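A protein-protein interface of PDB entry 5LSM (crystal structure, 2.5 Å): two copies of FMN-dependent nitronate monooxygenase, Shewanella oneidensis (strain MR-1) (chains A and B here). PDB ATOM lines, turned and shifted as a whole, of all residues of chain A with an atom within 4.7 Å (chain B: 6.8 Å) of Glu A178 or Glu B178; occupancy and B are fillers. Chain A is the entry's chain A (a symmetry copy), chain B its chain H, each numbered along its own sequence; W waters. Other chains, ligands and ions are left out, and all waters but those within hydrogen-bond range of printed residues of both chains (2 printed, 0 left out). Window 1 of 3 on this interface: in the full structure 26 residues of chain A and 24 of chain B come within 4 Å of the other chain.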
ATOM      1  N   GLY A 176      31.492 -13.141  30.539  1.00  0.00           N
ATOM      2  CA  GLY A 176      30.320 -12.564  29.943  1.00  0.00           C
ATOM      3  C   GLY A 176      30.659 -11.378  29.078  1.00  0.00           C
ATOM      4  O   GLY A 176      31.691 -10.740  29.263  1.00  0.00           O
ATOM      5  N   LEU A 177      29.738 -11.053  28.176  1.00  0.00           N
ATOM      6  CA  LEU A 177      29.849  -9.884  27.315  1.00  0.00           C
ATOM      7  C   LEU A 177      30.051  -8.580  28.070  1.00  0.00           C
ATOM      8  O   LEU A 177      30.502  -7.613  27.482  1.00  0.00           O
ATOM      9  CB  LEU A 177      28.603  -9.761  26.407  1.00  0.00           C
ATOM     10  CG  LEU A 177      28.521 -10.688  25.183  1.00  0.00           C
ATOM     11  CD1 LEU A 177      27.222 -10.468  24.439  1.00  0.00           C
ATOM     12  CD2 LEU A 177      29.688 -10.442  24.257  1.00  0.00           C
ATOM     13  N   GLU A 178      29.692  -8.541  29.355  1.00  0.00           N
ATOM     14  CA  GLU A 178      29.874  -7.335  30.188  1.00  0.00           C
ATOM     15  C   GLU A 178      31.370  -6.982  30.376  1.00  0.00           C
ATOM     16  O   GLU A 178      31.716  -5.840  30.703  1.00  0.00           O
ATOM     17  CB  GLU A 178      29.225  -7.540  31.566  1.00  0.00           C
ATOM     18  CG  GLU A 178      27.686  -7.519  31.594  1.00  0.00           C
ATOM     19  CD  GLU A 178      27.014  -8.898  31.501  1.00  0.00           C
ATOM     20  OE1 GLU A 178      27.583  -9.845  30.879  1.00  0.00           O
ATOM     21  OE2 GLU A 178      25.888  -9.036  32.044  1.00  0.00           O
ATOM     22  N   ALA A 179      32.245  -7.973  30.232  1.00  0.00           N
ATOM     23  CA  ALA A 179      33.673  -7.790  30.472  1.00  0.00           C
ATOM     24  C   ALA A 179      34.278  -6.683  29.630  1.00  0.00           C
ATOM     25  O   ALA A 179      33.935  -6.513  28.455  1.00  0.00           O
ATOM     26  CB  ALA A 179      34.421  -9.091  30.225  1.00  0.00           C
ATOM     27  N   GLY A 180      35.216  -5.963  30.238  1.00  0.00           N
ATOM     28  CA  GLY A 180      36.132  -5.084  29.506  1.00  0.00           C
ATOM     29  C   GLY A 180      37.216  -5.849  28.756  1.00  0.00           C
ATOM     30  O   GLY A 180      37.429  -7.031  29.007  1.00  0.00           O
ATOM     31  N   GLY A 196      25.780 -12.966  28.086  1.00  0.00           N
ATOM     32  CA  GLY A 196      26.076 -12.198  29.284  1.00  0.00           C
ATOM     33  C   GLY A 196      26.419 -13.068  30.472  1.00  0.00           C
ATOM     34  O   GLY A 196      26.033 -14.244  30.541  1.00  0.00           O
ATOM     35  N   THR A 197      27.096 -12.472  31.445  1.00  0.00           N
ATOM     36  CA  THR A 197      27.544 -13.211  32.624  1.00  0.00           C
ATOM     37  C   THR A 197      26.431 -14.041  33.262  1.00  0.00           C
ATOM     38  O   THR A 197      26.651 -15.195  33.638  1.00  0.00           O
ATOM     39  CB  THR A 197      28.161 -12.272  33.667  1.00  0.00           C
ATOM     40  OG1 THR A 197      29.487 -11.934  33.260  1.00  0.00           O
ATOM     41  CG2 THR A 197      28.210 -12.947  35.058  1.00  0.00           C
ATOM     42  N   PHE A 198      25.243 -13.457  33.350  1.00  0.00           N
ATOM     43  CA  PHE A 198      24.148 -14.028  34.114  1.00  0.00           C
ATOM     44  C   PHE A 198      23.704 -15.359  33.541  1.00  0.00           C
ATOM     45  O   PHE A 198      23.186 -16.207  34.259  1.00  0.00           O
ATOM     46  CB  PHE A 198      22.955 -13.069  34.127  1.00  0.00           C
ATOM     47  CG  PHE A 198      22.063 -13.243  35.302  1.00  0.00           C
ATOM     48  CD1 PHE A 198      22.484 -12.847  36.571  1.00  0.00           C
ATOM     49  CD2 PHE A 198      20.799 -13.778  35.155  1.00  0.00           C
ATOM     50  CE1 PHE A 198      21.662 -13.012  37.665  1.00  0.00           C
ATOM     51  CE2 PHE A 198      19.967 -13.924  36.245  1.00  0.00           C
ATOM     52  CZ  PHE A 198      20.405 -13.560  37.501  1.00  0.00           C
ATOM     53  N   SER A 199      23.854 -15.500  32.228  1.00  0.00           N
ATOM     54  CA  SER A 199      23.490 -16.725  31.536  1.00  0.00           C
ATOM     55  C   SER A 199      24.677 -17.644  31.218  1.00  0.00           C
ATOM     56  O   SER A 199      24.510 -18.847  31.171  1.00  0.00           O
ATOM     57  CB  SER A 199      22.733 -16.368  30.264  1.00  0.00           C
ATOM     58  OG  SER A 199      21.470 -15.829  30.611  1.00  0.00           O
ATOM     59  N   GLY A 216      33.253 -10.630  34.169  1.00  0.00           N
ATOM     60  CA  GLY A 216      32.332  -9.755  33.439  1.00  0.00           C
ATOM     61  C   GLY A 216      31.335  -9.058  34.363  1.00  0.00           C
ATOM     62  O   GLY A 216      30.286  -9.593  34.665  1.00  0.00           O
ATOM     63  N   GLY A 217      31.700  -7.882  34.859  1.00  0.00           N
ATOM     64  CA  GLY A 217      30.787  -7.060  35.654  1.00  0.00           C
ATOM     65  C   GLY A 217      30.858  -7.299  37.149  1.00  0.00           C
ATOM     66  O   GLY A 217      29.970  -6.882  37.882  1.00  0.00           O
ATOM     67  N   ARG A 277      35.872  -4.599  24.302  1.00  0.00           N
ATOM     68  CA  ARG A 277      34.905  -3.653  24.872  1.00  0.00           C
ATOM     69  C   ARG A 277      35.617  -2.447  25.462  1.00  0.00           C
ATOM     70  O   ARG A 277      36.486  -2.582  26.341  1.00  0.00           O
ATOM     71  CB  ARG A 277      34.027  -4.314  25.947  1.00  0.00           C
ATOM     72  CG  ARG A 277      32.968  -3.380  26.541  1.00  0.00           C
ATOM     73  CD  ARG A 277      32.078  -4.062  27.602  1.00  0.00           C
ATOM     74  NE  ARG A 277      31.216  -5.081  26.999  1.00  0.00           N
ATOM     75  CZ  ARG A 277      30.144  -4.833  26.237  1.00  0.00           C
ATOM     76  NH1 ARG A 277      29.716  -3.596  26.045  1.00  0.00           N
ATOM     77  NH2 ARG A 277      29.499  -5.831  25.670  1.00  0.00           N
ATOM     78  N   GLY A 325      34.423  -2.454  31.273  1.00  0.00           N
ATOM     79  CA  GLY A 325      33.250  -3.309  31.225  1.00  0.00           C
ATOM     80  C   GLY A 325      31.986  -2.495  31.349  1.00  0.00           C
ATOM     81  O   GLY A 325      32.029  -1.286  31.371  1.00  0.00           O
ATOM     82  N   GLN A 326      30.859  -3.166  31.452  1.00  0.00           N
ATOM     83  CA  GLN A 326      29.579  -2.487  31.432  1.00  0.00           C
ATOM     84  C   GLN A 326      29.152  -1.984  32.793  1.00  0.00           C
ATOM     85  O   GLN A 326      28.059  -1.424  32.933  1.00  0.00           O
ATOM     86  CB  GLN A 326      28.495  -3.405  30.886  1.00  0.00           C
ATOM     87  CG  GLN A 326      28.545  -3.599  29.389  1.00  0.00           C
ATOM     88  CD  GLN A 326      27.310  -4.325  28.869  1.00  0.00           C
ATOM     89  OE1 GLN A 326      26.825  -5.286  29.482  1.00  0.00           O
ATOM     90  NE2 GLN A 326      26.791  -3.860  27.750  1.00  0.00           N
ATOM     91  N   GLN B 175      15.200  -5.153  31.930  1.00  0.00           N
ATOM     92  CA  GLN B 175      15.487  -6.319  31.110  1.00  0.00           C
ATOM     93  C   GLN B 175      16.849  -6.231  30.503  1.00  0.00           C
ATOM     94  O   GLN B 175      17.141  -5.326  29.672  1.00  0.00           O
ATOM     95  CB  GLN B 175      14.413  -6.659  30.061  1.00  0.00           C
ATOM     96  CG  GLN B 175      13.988  -5.539  29.173  1.00  0.00           C
ATOM     97  CD  GLN B 175      13.705  -5.991  27.750  1.00  0.00           C
ATOM     98  OE1 GLN B 175      13.957  -5.253  26.804  1.00  0.00           O
ATOM     99  NE2 GLN B 175      13.122  -7.175  27.600  1.00  0.00           N
ATOM    100  N   GLY B 176      17.691  -7.151  30.980  1.00  0.00           N
ATOM    101  CA  GLY B 176      18.992  -7.389  30.415  1.00  0.00           C
ATOM    102  C   GLY B 176      18.889  -7.924  29.011  1.00  0.00           C
ATOM    103  O   GLY B 176      17.852  -8.409  28.595  1.00  0.00           O
ATOM    104  N   LEU B 177      20.004  -7.885  28.302  1.00  0.00           N
ATOM    105  CA  LEU B 177      20.060  -8.377  26.945  1.00  0.00           C
ATOM    106  C   LEU B 177      19.747  -9.865  26.834  1.00  0.00           C
ATOM    107  O   LEU B 177      19.385 -10.347  25.760  1.00  0.00           O
ATOM    108  CB  LEU B 177      21.444  -8.095  26.347  1.00  0.00           C
ATOM    109  CG  LEU B 177      21.708  -6.689  25.802  1.00  0.00           C
ATOM    110  CD1 LEU B 177      23.137  -6.611  25.301  1.00  0.00           C
ATOM    111  CD2 LEU B 177      20.739  -6.367  24.687  1.00  0.00           C
ATOM    112  N   GLU B 178      19.916 -10.606  27.915  1.00  0.00           N
ATOM    113  CA  GLU B 178      19.620 -12.044  27.891  1.00  0.00           C
ATOM    114  C   GLU B 178      18.142 -12.332  27.630  1.00  0.00           C
ATOM    115  O   GLU B 178      17.804 -13.410  27.172  1.00  0.00           O
ATOM    116  CB  GLU B 178      20.027 -12.698  29.204  1.00  0.00           C
ATOM    117  CG  GLU B 178      21.530 -12.656  29.478  1.00  0.00           C
ATOM    118  CD  GLU B 178      21.975 -11.372  30.164  1.00  0.00           C
ATOM    119  OE1 GLU B 178      21.132 -10.467  30.331  1.00  0.00           O
ATOM    120  OE2 GLU B 178      23.159 -11.274  30.556  1.00  0.00           O
ATOM    121  N   ALA B 179      17.263 -11.380  27.944  1.00  0.00           N
ATOM    122  CA  ALA B 179      15.817 -11.595  27.841  1.00  0.00           C
ATOM    123  C   ALA B 179      15.356 -12.099  26.462  1.00  0.00           C
ATOM    124  O   ALA B 179      15.925 -11.753  25.441  1.00  0.00           O
ATOM    125  CB  ALA B 179      15.078 -10.316  28.210  1.00  0.00           C
ATOM    126  N   GLY B 180      14.318 -12.926  26.449  1.00  0.00           N
ATOM    127  CA  GLY B 180      13.623 -13.288  25.201  1.00  0.00           C
ATOM    128  C   GLY B 180      12.634 -12.230  24.754  1.00  0.00           C
ATOM    129  O   GLY B 180      12.276 -11.334  25.510  1.00  0.00           O
ATOM    130  N   GLY B 181      12.268 -12.277  23.485  1.00  0.00           N
ATOM    131  CA  GLY B 181      11.334 -11.309  22.934  1.00  0.00           C
ATOM    132  C   GLY B 181      11.922  -9.940  22.665  1.00  0.00           C
ATOM    133  O   GLY B 181      13.143  -9.732  22.721  1.00  0.00           O
ATOM    134  N   ARG B 183      13.182  -6.262  22.640  1.00  0.00           N
ATOM    135  CA  ARG B 183      13.804  -5.258  23.475  1.00  0.00           C
ATOM    136  C   ARG B 183      12.795  -4.146  23.759  1.00  0.00           C
ATOM    137  O   ARG B 183      12.188  -3.620  22.847  1.00  0.00           O
ATOM    138  CB  ARG B 183      15.041  -4.681  22.756  1.00  0.00           C
ATOM    139  CG  ARG B 183      16.087  -5.714  22.344  1.00  0.00           C
ATOM    140  CD  ARG B 183      16.481  -6.598  23.512  1.00  0.00           C
ATOM    141  NE  ARG B 183      16.985  -5.816  24.636  1.00  0.00           N
ATOM    142  CZ  ARG B 183      17.047  -6.241  25.896  1.00  0.00           C
ATOM    143  NH1 ARG B 183      16.611  -7.449  26.237  1.00  0.00           N
ATOM    144  NH2 ARG B 183      17.527  -5.443  26.822  1.00  0.00           N
ATOM    145  N   LEU B 195      22.400  -3.502  28.136  1.00  0.00           N
ATOM    146  CA  LEU B 195      23.215  -4.143  29.151  1.00  0.00           C
ATOM    147  C   LEU B 195      22.704  -5.537  29.524  1.00  0.00           C
ATOM    148  O   LEU B 195      21.493  -5.783  29.593  1.00  0.00           O
ATOM    149  CB  LEU B 195      23.241  -3.267  30.398  1.00  0.00           C
ATOM    150  CG  LEU B 195      23.942  -1.907  30.287  1.00  0.00           C
ATOM    151  CD1 LEU B 195      24.036  -1.264  31.662  1.00  0.00           C
ATOM    152  CD2 LEU B 195      25.332  -2.063  29.707  1.00  0.00           C
ATOM    153  N   GLY B 196      23.629  -6.457  29.778  1.00  0.00           N
ATOM    154  CA  GLY B 196      23.264  -7.725  30.399  1.00  0.00           C
ATOM    155  C   GLY B 196      22.783  -7.538  31.832  1.00  0.00           C
ATOM    156  O   GLY B 196      23.230  -6.621  32.526  1.00  0.00           O
ATOM    157  N   THR B 197      21.874  -8.411  32.259  1.00  0.00           N
ATOM    158  CA  THR B 197      21.216  -8.341  33.561  1.00  0.00           C
ATOM    159  C   THR B 197      22.181  -8.082  34.729  1.00  0.00           C
ATOM    160  O   THR B 197      21.947  -7.210  35.581  1.00  0.00           O
ATOM    161  CB  THR B 197      20.500  -9.675  33.829  1.00  0.00           C
ATOM    162  OG1 THR B 197      19.515  -9.902  32.812  1.00  0.00           O
ATOM    163  CG2 THR B 197      19.843  -9.686  35.212  1.00  0.00           C
ATOM    164  N   PHE B 198      23.265  -8.839  34.749  1.00  0.00           N
ATOM    165  CA  PHE B 198      24.282  -8.746  35.802  1.00  0.00           C
ATOM    166  C   PHE B 198      24.836  -7.333  36.001  1.00  0.00           C
ATOM    167  O   PHE B 198      25.314  -6.999  37.099  1.00  0.00           O
ATOM    168  CB  PHE B 198      25.438  -9.690  35.492  1.00  0.00           C
ATOM    169  CG  PHE B 198      26.308  -9.971  36.659  1.00  0.00           C
ATOM    170  CD1 PHE B 198      25.906 -10.868  37.624  1.00  0.00           C
ATOM    171  CD2 PHE B 198      27.554  -9.378  36.768  1.00  0.00           C
ATOM    172  CE1 PHE B 198      26.712 -11.161  38.699  1.00  0.00           C
ATOM    173  CE2 PHE B 198      28.376  -9.664  37.841  1.00  0.00           C
ATOM    174  CZ  PHE B 198      27.950 -10.555  38.813  1.00  0.00           C
ATOM    175  N   SER B 199      24.783  -6.516  34.955  1.00  0.00           N
ATOM    176  CA  SER B 199      25.266  -5.141  35.039  1.00  0.00           C
ATOM    177  C   SER B 199      24.153  -4.105  35.066  1.00  0.00           C
ATOM    178  O   SER B 199      24.290  -3.061  35.704  1.00  0.00           O
ATOM    179  CB  SER B 199      26.228  -4.847  33.889  1.00  0.00           C
ATOM    180  OG  SER B 199      27.519  -5.340  34.200  1.00  0.00           O
ATOM    181  N   LEU B 200      23.078  -4.364  34.341  1.00  0.00           N
ATOM    182  CA  LEU B 200      21.935  -3.475  34.338  1.00  0.00           C
ATOM    183  C   LEU B 200      21.235  -3.462  35.680  1.00  0.00           C
ATOM    184  O   LEU B 200      20.888  -2.399  36.197  1.00  0.00           O
ATOM    185  CB  LEU B 200      20.940  -3.907  33.272  1.00  0.00           C
ATOM    186  CG  LEU B 200      19.667  -3.083  33.224  1.00  0.00           C
ATOM    187  CD1 LEU B 200      19.923  -1.743  32.531  1.00  0.00           C
ATOM    188  CD2 LEU B 200      18.599  -3.893  32.507  1.00  0.00           C
ATOM    189  N   ALA B 215      14.719  -8.945  34.979  1.00  0.00           N
ATOM    190  CA  ALA B 215      14.239  -9.689  33.804  1.00  0.00           C
ATOM    191  C   ALA B 215      15.375 -10.035  32.879  1.00  0.00           C
ATOM    192  O   ALA B 215      16.162  -9.160  32.507  1.00  0.00           O
ATOM    193  CB  ALA B 215      13.199  -8.871  33.048  1.00  0.00           C
ATOM    194  N   GLY B 216      15.411 -11.291  32.439  1.00  0.00           N
ATOM    195  CA  GLY B 216      16.400 -11.743  31.471  1.00  0.00           C
ATOM    196  C   GLY B 216      17.340 -12.770  32.046  1.00  0.00           C
ATOM    197  O   GLY B 216      18.322 -12.426  32.710  1.00  0.00           O
ATOM    198  N   GLY B 217      17.000 -14.039  31.851  1.00  0.00           N
ATOM    199  CA  GLY B 217      17.832 -15.158  32.306  1.00  0.00           C
ATOM    200  C   GLY B 217      17.525 -15.645  33.708  1.00  0.00           C
ATOM    201  O   GLY B 217      18.305 -16.405  34.294  1.00  0.00           O
ATOM    202  N   ILE B 218      16.393 -15.216  34.257  1.00  0.00           N
ATOM    203  CA  ILE B 218      15.876 -15.828  35.479  1.00  0.00           C
ATOM    204  C   ILE B 218      15.036 -17.054  35.103  1.00  0.00           C
ATOM    205  O   ILE B 218      13.982 -16.933  34.472  1.00  0.00           O
ATOM    206  CB  ILE B 218      15.083 -14.818  36.347  1.00  0.00           C
ATOM    207  N   THR B 239      10.859 -17.087  29.398  1.00  0.00           N
ATOM    208  CA  THR B 239      11.344 -18.262  28.691  1.00  0.00           C
ATOM    209  C   THR B 239      11.097 -19.601  29.424  1.00  0.00           C
ATOM    210  O   THR B 239      10.691 -20.581  28.799  1.00  0.00           O
ATOM    211  CB  THR B 239      12.842 -18.116  28.329  1.00  0.00           C
ATOM    212  OG1 THR B 239      13.026 -17.003  27.437  1.00  0.00           O
ATOM    213  CG2 THR B 239      13.377 -19.380  27.655  1.00  0.00           C
ATOM    214  N   THR B 265      20.904 -17.826  20.091  1.00  0.00           N
ATOM    215  CA  THR B 265      19.849 -16.834  19.861  1.00  0.00           C
ATOM    216  C   THR B 265      20.501 -15.563  19.396  1.00  0.00           C
ATOM    217  O   THR B 265      21.703 -15.379  19.570  1.00  0.00           O
ATOM    218  CB  THR B 265      19.054 -16.504  21.155  1.00  0.00           C
ATOM    219  OG1 THR B 265      19.929 -15.933  22.145  1.00  0.00           O
ATOM    220  CG2 THR B 265      18.390 -17.747  21.723  1.00  0.00           C
ATOM    221  N   ARG B 277      14.824 -10.977  20.730  1.00  0.00           N
ATOM    222  CA  ARG B 277      15.727 -12.132  20.841  1.00  0.00           C
ATOM    223  C   ARG B 277      14.991 -13.428  20.516  1.00  0.00           C
ATOM    224  O   ARG B 277      14.027 -13.782  21.192  1.00  0.00           O
ATOM    225  CB  ARG B 277      16.337 -12.210  22.229  1.00  0.00           C
ATOM    226  CG  ARG B 277      17.227 -13.429  22.427  1.00  0.00           C
ATOM    227  CD  ARG B 277      17.963 -13.367  23.757  1.00  0.00           C
ATOM    228  NE  ARG B 277      18.864 -12.229  23.782  1.00  0.00           N
ATOM    229  CZ  ARG B 277      20.020 -12.173  23.122  1.00  0.00           C
ATOM    230  NH1 ARG B 277      20.464 -13.223  22.450  1.00  0.00           N
ATOM    231  NH2 ARG B 277      20.751 -11.071  23.166  1.00  0.00           N
ATOM    232  N   CYS B 324      13.012 -16.488  22.785  1.00  0.00           N
ATOM    233  CA  CYS B 324      13.712 -17.335  23.733  1.00  0.00           C
ATOM    234  C   CYS B 324      14.901 -16.566  24.288  1.00  0.00           C
ATOM    235  O   CYS B 324      15.599 -15.862  23.548  1.00  0.00           O
ATOM    236  CB  CYS B 324      14.201 -18.611  23.052  1.00  0.00           C
ATOM    237  SG  CYS B 324      15.093 -19.769  24.142  1.00  0.00           S
ATOM    238  N   GLY B 325      15.095 -16.651  25.600  1.00  0.00           N
ATOM    239  CA  GLY B 325      16.199 -15.973  26.252  1.00  0.00           C
ATOM    240  C   GLY B 325      17.492 -16.744  26.086  1.00  0.00           C
ATOM    241  O   GLY B 325      17.519 -17.821  25.476  1.00  0.00           O
ATOM    242  N   GLN B 326      18.583 -16.173  26.590  1.00  0.00           N
ATOM    243  CA  GLN B 326      19.886 -16.785  26.417  1.00  0.00           C
ATOM    244  C   GLN B 326      20.129 -17.937  27.380  1.00  0.00           C
ATOM    245  O   GLN B 326      21.166 -18.613  27.283  1.00  0.00           O
ATOM    246  CB  GLN B 326      20.991 -15.770  26.570  1.00  0.00           C
ATOM    247  CG  GLN B 326      21.104 -14.812  25.408  1.00  0.00           C
ATOM    248  CD  GLN B 326      22.405 -14.041  25.462  1.00  0.00           C
ATOM    249  OE1 GLN B 326      22.767 -13.462  26.500  1.00  0.00           O
ATOM    250  NE2 GLN B 326      23.174 -14.133  24.395  1.00  0.00           N
ATOM    251  N   ASN B 327      19.148 -18.214  28.242  1.00  0.00           N
ATOM    252  CA  ASN B 327      19.175 -19.408  29.060  1.00  0.00           C
ATOM    253  C   ASN B 327      17.868 -20.224  28.968  1.00  0.00           C
ATOM    254  O   ASN B 327      16.899 -19.926  29.678  1.00  0.00           O
ATOM    255  CB  ASN B 327      19.483 -19.031  30.513  1.00  0.00           C
ATOM    256  CG  ASN B 327      19.883 -20.223  31.349  1.00  0.00           C
ATOM    257  OD1 ASN B 327      19.481 -21.351  31.070  1.00  0.00           O
ATOM    258  ND2 ASN B 327      20.680 -19.979  32.394  1.00  0.00           N
HETATM  259  O   HOH W   1      27.643  -5.638  37.132  1.00  0.00           O
HETATM  260  O   HOH W   2      20.581 -16.938  33.175  1.00  0.00           O
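Glu B178 touches Glu A178 (OE2 to OE2, 3.8 Å).
Phe B198 touches Glu A178.
Gly A196 touches Glu B178.
Phe B198 touches Thr A197.
Ser A199 touches Glu B178.
Ser A199 touches Asn B327 (OG to CB, 3.8 Å).
Gly A216 touches Phe B198.
CE2 of Phe B198 touches O of Gly A217, at 3.2 Å.
Ser B199 touches Gly A217 (OG to CA, 3.97 Å).
Ser B199 touches Gln A326.
Glu A178 touches Gly B196, and with the chains exchanged Gly A196 touches Glu B178.
Thr A197 touches Phe B198, but with the chains exchanged Phe A198 does not touch Thr B197 (4.2 Å).
Phe A198 touches Gly B217, and with the chains exchanged Gly A217 touches Phe B198.
Gln A326 touches Ser B199, but with the chains exchanged Ser A199 does not touch Gln B326 (4.05 Å).
Of the 17 pairs that touch across the chains among the printed residues, 11 have their exchanged pair printed and touching as well.
Glu A178 touches four residues of chain B.
Of the printed residues of chain A, Glu B178 touches Glu A178 (3.8 Å), Gly A196 (3.3 Å) and Ser A199 (3.4 Å).
Of the printed residues of chain A, Gly B216 touches Phe A198.
Of the printed residues of chain B, Gln A326 touches Leu B195 (3.0 Å), Gly B196 (3.4 Å) and Ser B199 (3.96 Å).
Of the printed residues of chain B, Gly A217 touches Phe B198 (3.2 Å) and Ser B199 (3.97 Å).
Cys B324 touches none of the printed residues of chain A.
The nearest printed residue of chain A that does not touch Glu B178 is Phe A198 (4.002 Å).
The nearest printed residue of chain A that does not touch Phe B198 is Phe A198 (4.1 Å).
Water W2 lies within hydrogen-bond range of the backbone carbonyl oxygen (O) of Gly B217, the backbone carbonyl oxygen (O) of Phe A198, the side-chain hydroxyl (OG) of Ser A199 and the side-chain amide nitrogen (ND2) of Asn B327.
Water W1 lies within hydrogen-bond range of O of Phe B198 (2.7 Å), O of Gly A217 (2.7 Å) and OG of Ser B199 (2.9 Å).
Printed residues of chain A that touch a printed residue of chain B: Glu A178, Gly A196, Thr A197, Phe A198, Ser A199, Gly A216, Gly A217 and Gln A326.
Hydrophobic or aromatic side chains of chain A that line the printed part of chain B: Phe A198.
Printed residues of chain B that touch a printed residue of chain A: Glu B178, Leu B195, Gly B196, Phe B198, Ser B199, Gly B216, Gly B217, Gln B326 and Asn B327.
Hydrophobic or aromatic side chains of chain B within 4 Å of the printed part of chain A: Leu B195 and Phe B198.
Among the printed residues, no Asp or Glu carboxylate lies within 4 Å of a Lys or Arg side-chain nitrogen of the other chain.
NE2 of Gln A326 sits close to NH1 of Arg A277 (3.4 Å).
O of Leu B195 sits at hydrogen-bond distance from N of Leu B177 (2.9 Å).
N of Gln B326 sits at hydrogen-bond distance from O of Glu B178, 2.9 Å away.
O of Gly A216 sits at hydrogen-bond distance from OG1 of Thr A197 (2.8 Å).
N of Thr A197 is in hydrogen-bond range of OE1 of Glu A178 (2.7 Å).
The side-chain carboxylate of Glu B178 is in hydrogen-bond range of the backbone NH of Thr B197, 2.9 Å away.
The backbone NH (N) of Gly B196 is in hydrogen-bond range of the side-chain amide oxygen (OE1) of Gln A326 (3.4 Å).
The side-chain amide oxygen of Gln B326 sits at hydrogen-bond distance from the backbone NH of Gly A196 (3.4 Å).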
